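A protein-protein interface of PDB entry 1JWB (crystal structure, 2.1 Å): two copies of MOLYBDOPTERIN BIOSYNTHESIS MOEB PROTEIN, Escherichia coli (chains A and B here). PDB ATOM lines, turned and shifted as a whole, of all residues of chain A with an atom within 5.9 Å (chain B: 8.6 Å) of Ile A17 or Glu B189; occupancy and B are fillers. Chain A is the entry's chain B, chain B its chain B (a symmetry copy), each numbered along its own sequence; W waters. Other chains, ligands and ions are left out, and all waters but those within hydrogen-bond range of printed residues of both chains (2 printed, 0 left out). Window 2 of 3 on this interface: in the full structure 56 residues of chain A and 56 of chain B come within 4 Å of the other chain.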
ATOM      1  N   TYR A  12      -5.676   5.953 -22.439  1.00  0.00           N
ATOM      2  CA  TYR A  12      -5.546   5.568 -21.030  1.00  0.00           C
ATOM      3  C   TYR A  12      -6.358   4.366 -20.677  1.00  0.00           C
ATOM      4  O   TYR A  12      -6.550   4.024 -19.529  1.00  0.00           O
ATOM      5  CB  TYR A  12      -5.947   6.722 -20.156  1.00  0.00           C
ATOM      6  CG  TYR A  12      -5.206   8.010 -20.404  1.00  0.00           C
ATOM      7  CD1 TYR A  12      -5.896   9.211 -20.517  1.00  0.00           C
ATOM      8  CD2 TYR A  12      -3.831   8.057 -20.451  1.00  0.00           C
ATOM      9  CE1 TYR A  12      -5.252  10.394 -20.682  1.00  0.00           C
ATOM     10  CE2 TYR A  12      -3.159   9.271 -20.581  1.00  0.00           C
ATOM     11  CZ  TYR A  12      -3.896  10.437 -20.680  1.00  0.00           C
ATOM     12  OH  TYR A  12      -3.304  11.624 -20.887  1.00  0.00           O
ATOM     13  N   ASN A  13      -6.776   3.643 -21.685  1.00  0.00           N
ATOM     14  CA  ASN A  13      -7.619   2.488 -21.409  1.00  0.00           C
ATOM     15  C   ASN A  13      -7.134   1.510 -20.327  1.00  0.00           C
ATOM     16  O   ASN A  13      -7.911   1.024 -19.495  1.00  0.00           O
ATOM     17  CB  ASN A  13      -7.827   1.759 -22.729  1.00  0.00           C
ATOM     18  CG  ASN A  13      -8.701   0.536 -22.580  1.00  0.00           C
ATOM     19  OD1 ASN A  13      -9.878   0.641 -22.242  1.00  0.00           O
ATOM     20  ND2 ASN A  13      -8.111  -0.631 -22.787  1.00  0.00           N
ATOM     21  N   ARG A  14      -5.859   1.161 -20.346  1.00  0.00           N
ATOM     22  CA  ARG A  14      -5.372   0.175 -19.388  1.00  0.00           C
ATOM     23  C   ARG A  14      -5.422   0.610 -17.924  1.00  0.00           C
ATOM     24  O   ARG A  14      -5.374  -0.218 -17.033  1.00  0.00           O
ATOM     25  CB  ARG A  14      -3.975  -0.236 -19.782  1.00  0.00           C
ATOM     26  CG  ARG A  14      -3.910  -0.945 -21.128  1.00  0.00           C
ATOM     27  CD  ARG A  14      -4.655  -2.296 -21.148  1.00  0.00           C
ATOM     28  NE  ARG A  14      -4.073  -3.231 -20.188  1.00  0.00           N
ATOM     29  CZ  ARG A  14      -3.273  -4.263 -20.505  1.00  0.00           C
ATOM     30  NH1 ARG A  14      -2.965  -4.529 -21.774  1.00  0.00           N
ATOM     31  NH2 ARG A  14      -2.794  -5.037 -19.542  1.00  0.00           N
ATOM     32  N   GLN A  15      -5.506   1.909 -17.672  1.00  0.00           N
ATOM     33  CA  GLN A  15      -5.656   2.381 -16.344  1.00  0.00           C
ATOM     34  C   GLN A  15      -7.129   2.465 -16.098  1.00  0.00           C
ATOM     35  O   GLN A  15      -7.595   2.120 -15.035  1.00  0.00           O
ATOM     36  CB  GLN A  15      -4.977   3.767 -16.182  1.00  0.00           C
ATOM     37  CG  GLN A  15      -3.487   3.609 -15.890  1.00  0.00           C
ATOM     38  CD  GLN A  15      -2.699   4.858 -15.998  1.00  0.00           C
ATOM     39  OE1 GLN A  15      -3.241   5.965 -16.080  1.00  0.00           O
ATOM     40  NE2 GLN A  15      -1.414   4.704 -16.009  1.00  0.00           N
ATOM     41  N   ILE A  16      -7.876   2.955 -17.085  1.00  0.00           N
ATOM     42  CA  ILE A  16      -9.305   3.180 -16.867  1.00  0.00           C
ATOM     43  C   ILE A  16     -10.021   1.898 -16.490  1.00  0.00           C
ATOM     44  O   ILE A  16     -10.946   1.930 -15.694  1.00  0.00           O
ATOM     45  CB  ILE A  16      -9.988   3.799 -18.093  1.00  0.00           C
ATOM     46  CG1 ILE A  16      -9.622   5.279 -18.240  1.00  0.00           C
ATOM     47  CG2 ILE A  16     -11.503   3.665 -17.985  1.00  0.00           C
ATOM     48  CD1 ILE A  16      -9.894   5.833 -19.661  1.00  0.00           C
ATOM     49  N   ILE A  17      -9.582   0.772 -17.037  1.00  0.00           N
ATOM     50  CA  ILE A  17     -10.255  -0.445 -16.701  1.00  0.00           C
ATOM     51  C   ILE A  17      -9.786  -1.098 -15.400  1.00  0.00           C
ATOM     52  O   ILE A  17     -10.230  -2.193 -15.123  1.00  0.00           O
ATOM     53  CB  ILE A  17     -10.155  -1.451 -17.864  1.00  0.00           C
ATOM     54  CG1 ILE A  17      -8.776  -2.059 -17.943  1.00  0.00           C
ATOM     55  CG2 ILE A  17     -10.597  -0.793 -19.158  1.00  0.00           C
ATOM     56  CD1 ILE A  17      -8.463  -2.671 -19.254  1.00  0.00           C
ATOM     57  N   LEU A  18      -8.882  -0.482 -14.635  1.00  0.00           N
ATOM     58  CA  LEU A  18      -8.509  -1.022 -13.339  1.00  0.00           C
ATOM     59  C   LEU A  18      -9.650  -0.691 -12.422  1.00  0.00           C
ATOM     60  O   LEU A  18     -10.142   0.446 -12.411  1.00  0.00           O
ATOM     61  CB  LEU A  18      -7.289  -0.363 -12.765  1.00  0.00           C
ATOM     62  CG  LEU A  18      -5.994  -0.558 -13.496  1.00  0.00           C
ATOM     63  CD1 LEU A  18      -4.925   0.402 -13.044  1.00  0.00           C
ATOM     64  CD2 LEU A  18      -5.620  -1.984 -13.223  1.00  0.00           C
ATOM     65  N   ARG A  19      -9.971  -1.665 -11.574  1.00  0.00           N
ATOM     66  CA  ARG A  19     -11.164  -1.655 -10.732  1.00  0.00           C
ATOM     67  C   ARG A  19     -11.559  -0.382 -10.043  1.00  0.00           C
ATOM     68  O   ARG A  19     -12.500   0.324 -10.462  1.00  0.00           O
ATOM     69  CB  ARG A  19     -11.058  -2.769  -9.700  1.00  0.00           C
ATOM     70  CG  ARG A  19     -12.302  -3.654  -9.603  1.00  0.00           C
ATOM     71  CD  ARG A  19     -11.957  -5.118  -9.261  1.00  0.00           C
ATOM     72  NE  ARG A  19     -11.549  -5.181  -7.863  1.00  0.00           N
ATOM     73  CZ  ARG A  19     -10.300  -5.054  -7.414  1.00  0.00           C
ATOM     74  NH1 ARG A  19      -9.254  -4.899  -8.219  1.00  0.00           N
ATOM     75  NH2 ARG A  19     -10.096  -5.093  -6.118  1.00  0.00           N
ATOM     76  N   ASP A  22     -10.953   3.544 -12.865  1.00  0.00           N
ATOM     77  CA  ASP A  22     -12.041   3.950 -13.695  1.00  0.00           C
ATOM     78  C   ASP A  22     -11.810   5.315 -14.291  1.00  0.00           C
ATOM     79  O   ASP A  22     -10.728   5.902 -14.185  1.00  0.00           O
ATOM     80  CB  ASP A  22     -13.254   3.939 -12.784  1.00  0.00           C
ATOM     81  CG  ASP A  22     -14.512   3.479 -13.460  1.00  0.00           C
ATOM     82  OD1 ASP A  22     -14.546   3.421 -14.702  1.00  0.00           O
ATOM     83  OD2 ASP A  22     -15.536   3.202 -12.800  1.00  0.00           O
ATOM     84  N   SER B  69      -3.048   2.828 -27.275  1.00  0.00           N
ATOM     85  CA  SER B  69      -3.187   2.313 -25.961  1.00  0.00           C
ATOM     86  C   SER B  69      -1.859   1.995 -25.283  1.00  0.00           C
ATOM     87  O   SER B  69      -1.777   2.076 -24.056  1.00  0.00           O
ATOM     88  CB  SER B  69      -3.989   1.048 -25.972  1.00  0.00           C
ATOM     89  OG  SER B  69      -3.939   0.574 -24.663  1.00  0.00           O
ATOM     90  N   ARG B  73       1.798   3.507 -21.251  1.00  0.00           N
ATOM     91  CA  ARG B  73       2.932   3.008 -20.475  1.00  0.00           C
ATOM     92  C   ARG B  73       4.232   2.668 -21.222  1.00  0.00           C
ATOM     93  O   ARG B  73       5.283   2.631 -20.609  1.00  0.00           O
ATOM     94  CB  ARG B  73       2.518   1.768 -19.662  1.00  0.00           C
ATOM     95  CG  ARG B  73       2.209   0.578 -20.527  1.00  0.00           C
ATOM     96  CD  ARG B  73       1.519  -0.507 -19.836  1.00  0.00           C
ATOM     97  NE  ARG B  73       1.334  -1.641 -20.724  1.00  0.00           N
ATOM     98  CZ  ARG B  73       0.399  -1.745 -21.619  1.00  0.00           C
ATOM     99  NH1 ARG B  73      -0.488  -0.789 -21.800  1.00  0.00           N
ATOM    100  NH2 ARG B  73       0.371  -2.813 -22.371  1.00  0.00           N
ATOM    101  N   ASP B 130       3.937 -11.228 -22.426  1.00  0.00           N
ATOM    102  CA  ASP B 130       2.666 -11.106 -21.756  1.00  0.00           C
ATOM    103  C   ASP B 130       1.842 -12.336 -21.838  1.00  0.00           C
ATOM    104  O   ASP B 130       0.679 -12.288 -21.820  1.00  0.00           O
ATOM    105  CB  ASP B 130       1.883  -9.942 -22.384  1.00  0.00           C
ATOM    106  CG  ASP B 130       1.735 -10.078 -23.901  1.00  0.00           C
ATOM    107  OD1 ASP B 130       2.092 -11.154 -24.445  1.00  0.00           O
ATOM    108  OD2 ASP B 130       1.323  -9.137 -24.630  1.00  0.00           O
ATOM    109  N   ASN B 131       2.468 -13.475 -21.962  1.00  0.00           N
ATOM    110  CA  ASN B 131       1.740 -14.731 -22.077  1.00  0.00           C
ATOM    111  C   ASN B 131       2.650 -15.897 -21.694  1.00  0.00           C
ATOM    112  O   ASN B 131       3.843 -15.917 -21.970  1.00  0.00           O
ATOM    113  CB  ASN B 131       1.109 -14.914 -23.477  1.00  0.00           C
ATOM    114  CG  ASN B 131       2.126 -15.069 -24.582  1.00  0.00           C
ATOM    115  OD1 ASN B 131       2.583 -16.182 -24.873  1.00  0.00           O
ATOM    116  ND2 ASN B 131       2.466 -13.954 -25.243  1.00  0.00           N
ATOM    117  N   ILE B 155       0.743  -6.910 -14.249  1.00  0.00           N
ATOM    118  CA  ILE B 155      -0.623  -6.671 -14.704  1.00  0.00           C
ATOM    119  C   ILE B 155      -1.258  -5.917 -13.543  1.00  0.00           C
ATOM    120  O   ILE B 155      -0.819  -6.029 -12.406  1.00  0.00           O
ATOM    121  CB  ILE B 155      -1.358  -7.997 -15.017  1.00  0.00           C
ATOM    122  CG1 ILE B 155      -2.611  -7.794 -15.887  1.00  0.00           C
ATOM    123  CG2 ILE B 155      -1.771  -8.702 -13.714  1.00  0.00           C
ATOM    124  CD1 ILE B 155      -2.351  -7.214 -17.238  1.00  0.00           C
ATOM    125  N   ARG B 156      -2.301  -5.168 -13.813  1.00  0.00           N
ATOM    126  CA  ARG B 156      -3.023  -4.499 -12.733  1.00  0.00           C
ATOM    127  C   ARG B 156      -2.136  -3.683 -11.821  1.00  0.00           C
ATOM    128  O   ARG B 156      -1.641  -2.629 -12.239  1.00  0.00           O
ATOM    129  CB  ARG B 156      -3.786  -5.546 -11.962  1.00  0.00           C
ATOM    130  CG  ARG B 156      -4.951  -6.047 -12.662  1.00  0.00           C
ATOM    131  CD  ARG B 156      -5.714  -7.109 -11.883  1.00  0.00           C
ATOM    132  NE  ARG B 156      -6.811  -7.670 -12.666  1.00  0.00           N
ATOM    133  CZ  ARG B 156      -6.778  -8.814 -13.349  1.00  0.00           C
ATOM    134  NH1 ARG B 156      -5.695  -9.598 -13.366  1.00  0.00           N
ATOM    135  NH2 ARG B 156      -7.853  -9.183 -14.027  1.00  0.00           N
ATOM    136  N   GLU B 189      -7.748  -6.075 -21.527  1.00  0.00           N
ATOM    137  CA  GLU B 189      -8.381  -7.221 -20.879  1.00  0.00           C
ATOM    138  C   GLU B 189      -8.398  -6.913 -19.377  1.00  0.00           C
ATOM    139  O   GLU B 189      -9.373  -6.424 -18.849  1.00  0.00           O
ATOM    140  CB  GLU B 189      -7.585  -8.501 -21.221  1.00  0.00           C
ATOM    141  CG  GLU B 189      -7.790  -8.987 -22.673  1.00  0.00           C
ATOM    142  CD  GLU B 189      -6.815 -10.077 -23.129  1.00  0.00           C
ATOM    143  OE1 GLU B 189      -6.320 -10.855 -22.283  1.00  0.00           O
ATOM    144  OE2 GLU B 189      -6.542 -10.160 -24.352  1.00  0.00           O
ATOM    145  N   ALA B 190      -7.296  -7.223 -18.703  1.00  0.00           N
ATOM    146  CA  ALA B 190      -7.024  -6.701 -17.392  1.00  0.00           C
ATOM    147  C   ALA B 190      -6.291  -5.369 -17.639  1.00  0.00           C
ATOM    148  O   ALA B 190      -5.578  -5.197 -18.628  1.00  0.00           O
ATOM    149  CB  ALA B 190      -6.162  -7.618 -16.661  1.00  0.00           C
ATOM    150  N   GLY B 191      -6.479  -4.425 -16.749  1.00  0.00           N
ATOM    151  CA  GLY B 191      -5.760  -3.185 -16.842  1.00  0.00           C
ATOM    152  C   GLY B 191      -4.325  -3.332 -16.374  1.00  0.00           C
ATOM    153  O   GLY B 191      -3.904  -4.404 -15.937  1.00  0.00           O
ATOM    154  N   VAL B 192      -3.576  -2.241 -16.461  1.00  0.00           N
ATOM    155  CA  VAL B 192      -2.236  -2.190 -15.882  1.00  0.00           C
ATOM    156  C   VAL B 192      -1.889  -0.718 -15.594  1.00  0.00           C
ATOM    157  O   VAL B 192      -2.127   0.162 -16.388  1.00  0.00           O
ATOM    158  CB  VAL B 192      -1.211  -2.908 -16.768  1.00  0.00           C
ATOM    159  CG1 VAL B 192      -1.123  -2.262 -18.166  1.00  0.00           C
ATOM    160  CG2 VAL B 192       0.168  -2.964 -16.080  1.00  0.00           C
ATOM    161  N   MET B 193      -1.420  -0.422 -14.383  1.00  0.00           N
ATOM    162  CA  MET B 193      -1.075   0.934 -14.061  1.00  0.00           C
ATOM    163  C   MET B 193       0.298   1.275 -14.589  1.00  0.00           C
ATOM    164  O   MET B 193       1.310   0.542 -14.395  1.00  0.00           O
ATOM    165  CB  MET B 193      -1.175   1.107 -12.558  1.00  0.00           C
ATOM    166  CG  MET B 193      -0.870   2.481 -12.057  1.00  0.00           C
ATOM    167  SD  MET B 193      -1.935   3.826 -12.555  1.00  0.00           S
ATOM    168  CE  MET B 193      -3.385   3.487 -11.590  1.00  0.00           C
HETATM  169  O   HOH W   1      -3.920   2.232 -22.088  1.00  0.00           O
HETATM  170  O   HOH W   2      -8.338  -4.561 -14.536  1.00  0.00           O
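NE of Arg A14 lies within hydrogen-bond range of O of Ala B190, 2.9 Å away. N of Val B192 is in hydrogen-bond range of O of Arg A14 (2.8 Å). The side-chain amide nitrogen (NE2) of Gln A15 lies within hydrogen-bond range of the side-chain sulfur (SD) of Met B193 (3.6 Å).
Water W1 lies within hydrogen-bond range of N of Arg A14 (2.8 Å), O of Ser B69 (2.9 Å) and N of Asn A13 (3.2 Å). Water W2 lies within hydrogen-bond range of N of Gly B191 (2.9 Å) and O of Ile A17 (3.1 Å).
Among the printed residues, merely in contact across the chains: Arg A14 with Ser B69, Arg A14 with Arg B73, Arg A14 with Ile B155, Arg A14 with Gly B191, Gln A15 with Val B192, Ile A17 with Glu B189, Ile A17 with Ala B190, Ile A17 with Gly B191, Leu A18 with Arg B156, Leu A18 with Gly B191, Leu A18 with Val B192 and Leu A18 with Met B193.
Of chain B, only Glu B189 (3.9 Å), Ala B190 (3.8 Å) and Gly B191 (3.4 Å) come within 4 Å of Ile A17. Glu B189 touches just one residue of chain A: Ile A17. Of the printed residues of chain A, Val B192 touches Arg A14 (2.8 Å), Gln A15 (3.7 Å) and Leu A18 (3.8 Å). Printed residues of chain A within 4 Å of Ser B69: Arg A14 (3.8 Å). Asn B131 touches none of the printed residues of chain A. Ile A16 touches none of the printed residues of chain B. The nearest residue of chain B that does not touch Ile A17 is Val B192 (5.4 Å).
No position is printed for both chains.
The backbone NH of Arg B156 lies within hydrogen-bond range of the backbone carbonyl oxygen of Gly B191 (2.8 Å). The backbone carbonyl oxygen (O) of Arg B156 is in hydrogen-bond range of the backbone NH (N) of Met B193.
Hydrophobic or aromatic side chains of chain B that line the printed part of chain A: Ile B155, Val B192 and Met B193. Of the 9 printed residues of chain A, 4 touch a printed residue of chain B. Printed residues of chain A that touch a printed residue of chain B: Arg A14, Gln A15, Ile A17 and Leu A18. Among the printed residues, 15 pairs touch across the chains. Among the printed residues, no Asp or Glu carboxylate lies within 4 Å of a Lys or Arg side-chain nitrogen of the other chain.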
